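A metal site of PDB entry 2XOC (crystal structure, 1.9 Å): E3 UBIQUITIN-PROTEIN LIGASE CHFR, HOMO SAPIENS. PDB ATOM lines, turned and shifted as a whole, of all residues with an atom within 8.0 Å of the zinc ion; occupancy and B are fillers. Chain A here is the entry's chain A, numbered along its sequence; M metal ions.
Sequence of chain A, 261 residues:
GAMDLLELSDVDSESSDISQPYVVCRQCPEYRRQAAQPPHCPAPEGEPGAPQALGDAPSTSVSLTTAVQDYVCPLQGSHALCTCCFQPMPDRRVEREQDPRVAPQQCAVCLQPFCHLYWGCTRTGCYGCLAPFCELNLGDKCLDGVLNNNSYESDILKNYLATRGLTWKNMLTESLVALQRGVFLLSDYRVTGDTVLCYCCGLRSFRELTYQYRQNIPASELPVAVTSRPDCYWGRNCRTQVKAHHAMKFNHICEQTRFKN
Of the 21 residues printed, 4 come within 4 Å of the zinc ion. Along chain A the residues within 4 Å of the zinc ion span positions 107 to 201.
The zinc ion is bound by the side-chain sulfur (SG) of Cys 110 (2.3 Å), the side-chain sulfur (SG) of Cys 107 (2.3 Å), the side-chain sulfur (SG) of Cys 201 (2.4 Å) and the side-chain sulfur (SG) of Cys 198 (2.4 Å). The zinc ion has four donor atoms within binding distance.
The backbone carbonyl oxygen (O) of Cys 110 lies within hydrogen-bond range of the side-chain amide nitrogen (NE2) of Gln 112. The side-chain sulfur of Cys 107 sits close to the backbone NH of Val 109 (3.3 Å). The backbone carbonyl oxygen (O) of Gln 112 sits at hydrogen-bond distance from the backbone NH (N) of Cys 107, 3.0 Å away. The side-chain sulfur (SG) of Cys 201 lies close to the guanidinium group (NH2) of Arg 204, at 3.3 Å. SG of Cys 198 lies close to N of Cys 200 (3.7 Å).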
ATOM      1  N   THR A  83      13.976   8.757   8.032  1.00  0.00           N
ATOM      2  CA  THR A  83      12.752   8.166   7.525  1.00  0.00           C
ATOM      3  C   THR A  83      12.885   7.796   6.050  1.00  0.00           C
ATOM      4  O   THR A  83      12.190   6.910   5.553  1.00  0.00           O
ATOM      5  CB  THR A  83      11.566   9.117   7.745  1.00  0.00           C
ATOM      6  OG1 THR A  83      11.430   9.400   9.141  1.00  0.00           O
ATOM      7  CG2 THR A  83      10.268   8.502   7.227  1.00  0.00           C
ATOM      8  N   GLN A 106      14.272  17.057  11.400  1.00  0.00           N
ATOM      9  CA  GLN A 106      12.915  16.561  11.232  1.00  0.00           C
ATOM     10  C   GLN A 106      12.062  17.496  10.380  1.00  0.00           C
ATOM     11  O   GLN A 106      12.327  18.693  10.286  1.00  0.00           O
ATOM     12  CB  GLN A 106      12.250  16.329  12.589  1.00  0.00           C
ATOM     13  CG  GLN A 106      11.954  17.600  13.395  1.00  0.00           C
ATOM     14  CD  GLN A 106      11.201  17.315  14.683  1.00  0.00           C
ATOM     15  OE1 GLN A 106      11.327  16.243  15.263  1.00  0.00           O
ATOM     16  NE2 GLN A 106      10.406  18.278  15.125  1.00  0.00           N
ATOM     17  N   CYS A 107      11.028  16.929   9.771  1.00  0.00           N
ATOM     18  CA  CYS A 107      10.050  17.711   9.029  1.00  0.00           C
ATOM     19  C   CYS A 107       9.163  18.462  10.027  1.00  0.00           C
ATOM     20  O   CYS A 107       8.692  17.874  11.002  1.00  0.00           O
ATOM     21  CB  CYS A 107       9.214  16.800   8.148  1.00  0.00           C
ATOM     22  SG  CYS A 107       7.805  17.600   7.350  1.00  0.00           S
ATOM     23  N   ALA A 108       8.952  19.748   9.771  1.00  0.00           N
ATOM     24  CA  ALA A 108       8.181  20.579  10.692  1.00  0.00           C
ATOM     25  C   ALA A 108       6.682  20.310  10.612  1.00  0.00           C
ATOM     26  O   ALA A 108       5.915  20.789  11.451  1.00  0.00           O
ATOM     27  CB  ALA A 108       8.469  22.045  10.411  1.00  0.00           C
ATOM     28  N   VAL A 109       6.275  19.527   9.621  1.00  0.00           N
ATOM     29  CA  VAL A 109       4.869  19.199   9.436  1.00  0.00           C
ATOM     30  C   VAL A 109       4.505  17.839  10.022  1.00  0.00           C
ATOM     31  O   VAL A 109       3.592  17.734  10.832  1.00  0.00           O
ATOM     32  CB  VAL A 109       4.474  19.224   7.939  1.00  0.00           C
ATOM     33  CG1 VAL A 109       3.049  18.694   7.752  1.00  0.00           C
ATOM     34  CG2 VAL A 109       4.611  20.634   7.376  1.00  0.00           C
ATOM     35  N   CYS A 110       5.233  16.792   9.610  1.00  0.00           N
ATOM     36  CA  CYS A 110       4.931  15.435  10.078  1.00  0.00           C
ATOM     37  C   CYS A 110       5.791  15.019  11.266  1.00  0.00           C
ATOM     38  O   CYS A 110       5.527  13.999  11.900  1.00  0.00           O
ATOM     39  CB  CYS A 110       5.088  14.431   8.936  1.00  0.00           C
ATOM     40  SG  CYS A 110       6.795  14.193   8.414  1.00  0.00           S
ATOM     41  N   LEU A 111       6.826  15.812  11.543  1.00  0.00           N
ATOM     42  CA  LEU A 111       7.674  15.624  12.716  1.00  0.00           C
ATOM     43  C   LEU A 111       8.528  14.346  12.671  1.00  0.00           C
ATOM     44  O   LEU A 111       9.102  13.942  13.682  1.00  0.00           O
ATOM     45  CB  LEU A 111       6.840  15.654  14.001  1.00  0.00           C
ATOM     46  CG  LEU A 111       5.981  16.902  14.201  1.00  0.00           C
ATOM     47  CD1 LEU A 111       5.316  16.881  15.557  1.00  0.00           C
ATOM     48  CD2 LEU A 111       6.801  18.165  14.038  1.00  0.00           C
ATOM     49  N   GLN A 112       8.607  13.704  11.498  1.00  0.00           N
ATOM     50  CA  GLN A 112       9.455  12.538  11.338  1.00  0.00           C
ATOM     51  C   GLN A 112      10.893  12.959  11.047  1.00  0.00           C
ATOM     52  O   GLN A 112      11.129  14.023  10.462  1.00  0.00           O
ATOM     53  CB  GLN A 112       8.926  11.614  10.238  1.00  0.00           C
ATOM     54  CG  GLN A 112       7.552  11.051  10.540  1.00  0.00           C
ATOM     55  CD  GLN A 112       7.483  10.395  11.915  1.00  0.00           C
ATOM     56  OE1 GLN A 112       8.238   9.469  12.215  1.00  0.00           O
ATOM     57  NE2 GLN A 112       6.566  10.881  12.750  1.00  0.00           N
ATOM     58  N   PRO A 113      11.879  12.138  11.454  1.00  0.00           N
ATOM     59  CA  PRO A 113      13.292  12.502  11.274  1.00  0.00           C
ATOM     60  C   PRO A 113      13.807  12.256   9.855  1.00  0.00           C
ATOM     61  O   PRO A 113      13.468  11.231   9.266  1.00  0.00           O
ATOM     62  CB  PRO A 113      14.005  11.575  12.260  1.00  0.00           C
ATOM     63  CG  PRO A 113      13.131  10.379  12.366  1.00  0.00           C
ATOM     64  CD  PRO A 113      11.711  10.862  12.161  1.00  0.00           C
ATOM     65  N   PHE A 114      14.600  13.191   9.342  1.00  0.00           N
ATOM     66  CA  PHE A 114      15.260  13.046   8.036  1.00  0.00           C
ATOM     67  C   PHE A 114      16.689  13.579   8.161  1.00  0.00           C
ATOM     68  O   PHE A 114      16.924  14.534   8.897  1.00  0.00           O
ATOM     69  CB  PHE A 114      14.509  13.810   6.953  1.00  0.00           C
ATOM     70  CG  PHE A 114      13.131  13.264   6.649  1.00  0.00           C
ATOM     71  CD1 PHE A 114      12.952  12.319   5.661  1.00  0.00           C
ATOM     72  CD2 PHE A 114      12.040  13.700   7.374  1.00  0.00           C
ATOM     73  CE1 PHE A 114      11.690  11.814   5.389  1.00  0.00           C
ATOM     74  CE2 PHE A 114      10.770  13.191   7.112  1.00  0.00           C
ATOM     75  CZ  PHE A 114      10.599  12.250   6.114  1.00  0.00           C
ATOM     76  N   CYS A 129      15.641  14.964   0.815  1.00  0.00           N
ATOM     77  CA  CYS A 129      14.367  14.678   1.472  1.00  0.00           C
ATOM     78  C   CYS A 129      13.926  15.680   2.528  1.00  0.00           C
ATOM     79  O   CYS A 129      12.823  15.572   3.064  1.00  0.00           O
ATOM     80  CB  CYS A 129      14.398  13.262   2.063  1.00  0.00           C
ATOM     81  SG  CYS A 129      15.852  12.950   3.105  1.00  0.00           S
ATOM     82  N   LEU A 130      14.770  16.662   2.830  1.00  0.00           N
ATOM     83  CA  LEU A 130      14.395  17.705   3.785  1.00  0.00           C
ATOM     84  C   LEU A 130      14.932  19.064   3.345  1.00  0.00           C
ATOM     85  O   LEU A 130      16.117  19.200   3.063  1.00  0.00           O
ATOM     86  CB  LEU A 130      14.935  17.361   5.173  1.00  0.00           C
ATOM     87  CG  LEU A 130      14.484  18.237   6.337  1.00  0.00           C
ATOM     88  CD1 LEU A 130      12.982  18.103   6.564  1.00  0.00           C
ATOM     89  CD2 LEU A 130      15.263  17.887   7.595  1.00  0.00           C
ATOM     90  N   ASP A 188      -2.514  21.856   5.372  1.00  0.00           N
ATOM     91  CA  ASP A 188      -1.512  22.151   6.396  1.00  0.00           C
ATOM     92  C   ASP A 188      -1.372  23.656   6.413  1.00  0.00           C
ATOM     93  O   ASP A 188      -0.400  24.221   5.913  1.00  0.00           O
ATOM     94  CB  ASP A 188      -0.185  21.467   6.063  1.00  0.00           C
ATOM     95  CG  ASP A 188      -0.297  19.955   6.038  1.00  0.00           C
ATOM     96  OD1 ASP A 188      -1.053  19.397   6.863  1.00  0.00           O
ATOM     97  OD2 ASP A 188       0.373  19.317   5.188  1.00  0.00           O
ATOM     98  N   VAL A 196      10.530  24.281   6.870  1.00  0.00           N
ATOM     99  CA  VAL A 196      11.405  23.148   6.593  1.00  0.00           C
ATOM    100  C   VAL A 196      10.602  21.856   6.656  1.00  0.00           C
ATOM    101  O   VAL A 196      10.152  21.450   7.730  1.00  0.00           O
ATOM    102  CB  VAL A 196      12.584  23.080   7.585  1.00  0.00           C
ATOM    103  CG1 VAL A 196      13.416  21.829   7.335  1.00  0.00           C
ATOM    104  CG2 VAL A 196      13.439  24.325   7.481  1.00  0.00           C
ATOM    105  N   LEU A 197      10.401  21.218   5.514  1.00  0.00           N
ATOM    106  CA  LEU A 197       9.573  20.012   5.456  1.00  0.00           C
ATOM    107  C   LEU A 197      10.189  18.916   4.600  1.00  0.00           C
ATOM    108  O   LEU A 197      11.203  19.114   3.941  1.00  0.00           O
ATOM    109  CB  LEU A 197       8.156  20.359   4.981  1.00  0.00           C
ATOM    110  CG  LEU A 197       7.963  21.340   3.819  1.00  0.00           C
ATOM    111  CD1 LEU A 197       8.573  20.812   2.528  1.00  0.00           C
ATOM    112  CD2 LEU A 197       6.476  21.640   3.619  1.00  0.00           C
ATOM    113  N   CYS A 198       9.564  17.742   4.622  1.00  0.00           N
ATOM    114  CA  CYS A 198      10.099  16.584   3.905  1.00  0.00           C
ATOM    115  C   CYS A 198       9.493  16.459   2.516  1.00  0.00           C
ATOM    116  O   CYS A 198       8.540  17.162   2.179  1.00  0.00           O
ATOM    117  CB  CYS A 198       9.860  15.303   4.703  1.00  0.00           C
ATOM    118  SG  CYS A 198       8.162  14.695   4.674  1.00  0.00           S
ATOM    119  N   TYR A 199      10.058  15.553   1.723  1.00  0.00           N
ATOM    120  CA  TYR A 199       9.578  15.328   0.371  1.00  0.00           C
ATOM    121  C   TYR A 199       8.073  15.069   0.300  1.00  0.00           C
ATOM    122  O   TYR A 199       7.369  15.726  -0.464  1.00  0.00           O
ATOM    123  CB  TYR A 199      10.334  14.167  -0.283  1.00  0.00           C
ATOM    124  CG  TYR A 199       9.649  13.638  -1.519  1.00  0.00           C
ATOM    125  CD1 TYR A 199       9.734  14.321  -2.722  1.00  0.00           C
ATOM    126  CD2 TYR A 199       8.916  12.468  -1.470  1.00  0.00           C
ATOM    127  CE1 TYR A 199       9.093  13.839  -3.851  1.00  0.00           C
ATOM    128  CE2 TYR A 199       8.276  11.986  -2.598  1.00  0.00           C
ATOM    129  CZ  TYR A 199       8.369  12.673  -3.775  1.00  0.00           C
ATOM    130  OH  TYR A 199       7.738  12.183  -4.898  1.00  0.00           O
ATOM    131  N   CYS A 200       7.588  14.129   1.095  1.00  0.00           N
ATOM    132  CA  CYS A 200       6.186  13.737   1.050  1.00  0.00           C
ATOM    133  C   CYS A 200       5.236  14.861   1.480  1.00  0.00           C
ATOM    134  O   CYS A 200       4.212  15.091   0.837  1.00  0.00           O
ATOM    135  CB  CYS A 200       5.937  12.469   1.872  1.00  0.00           C
ATOM    136  SG  CYS A 200       6.625  10.956   1.145  1.00  0.00           S
ATOM    137  N   CYS A 201       5.564  15.559   2.566  1.00  0.00           N
ATOM    138  CA  CYS A 201       4.746  16.675   3.013  1.00  0.00           C
ATOM    139  C   CYS A 201       4.765  17.833   2.017  1.00  0.00           C
ATOM    140  O   CYS A 201       3.745  18.469   1.762  1.00  0.00           O
ATOM    141  CB  CYS A 201       5.170  17.157   4.392  1.00  0.00           C
ATOM    142  SG  CYS A 201       4.759  16.005   5.725  1.00  0.00           S
ATOM    143  N   GLY A 202       5.940  18.114   1.468  1.00  0.00           N
ATOM    144  CA  GLY A 202       6.073  19.126   0.435  1.00  0.00           C
ATOM    145  C   GLY A 202       5.253  18.779  -0.799  1.00  0.00           C
ATOM    146  O   GLY A 202       4.569  19.628  -1.367  1.00  0.00           O
ATOM    147  N   ARG A 204       2.645  16.896  -0.957  1.00  0.00           N
ATOM    148  CA  ARG A 204       1.236  16.991  -0.613  1.00  0.00           C
ATOM    149  C   ARG A 204       0.710  18.408  -0.773  1.00  0.00           C
ATOM    150  O   ARG A 204      -0.366  18.628  -1.330  1.00  0.00           O
ATOM    151  CB  ARG A 204       0.994  16.481   0.817  1.00  0.00           C
ATOM    152  CG  ARG A 204      -0.475  16.414   1.206  1.00  0.00           C
ATOM    153  CD  ARG A 204      -0.682  15.671   2.516  1.00  0.00           C
ATOM    154  NE  ARG A 204      -0.034  16.343   3.651  1.00  0.00           N
ATOM    155  CZ  ARG A 204       1.062  15.900   4.249  1.00  0.00           C
ATOM    156  NH1 ARG A 204       1.654  14.791   3.829  1.00  0.00           N
ATOM    157  NH2 ARG A 204       1.569  16.573   5.272  1.00  0.00           N
HETATM  158 ZN    ZN M   1       6.926  15.578   6.555  1.00  0.00          ZN
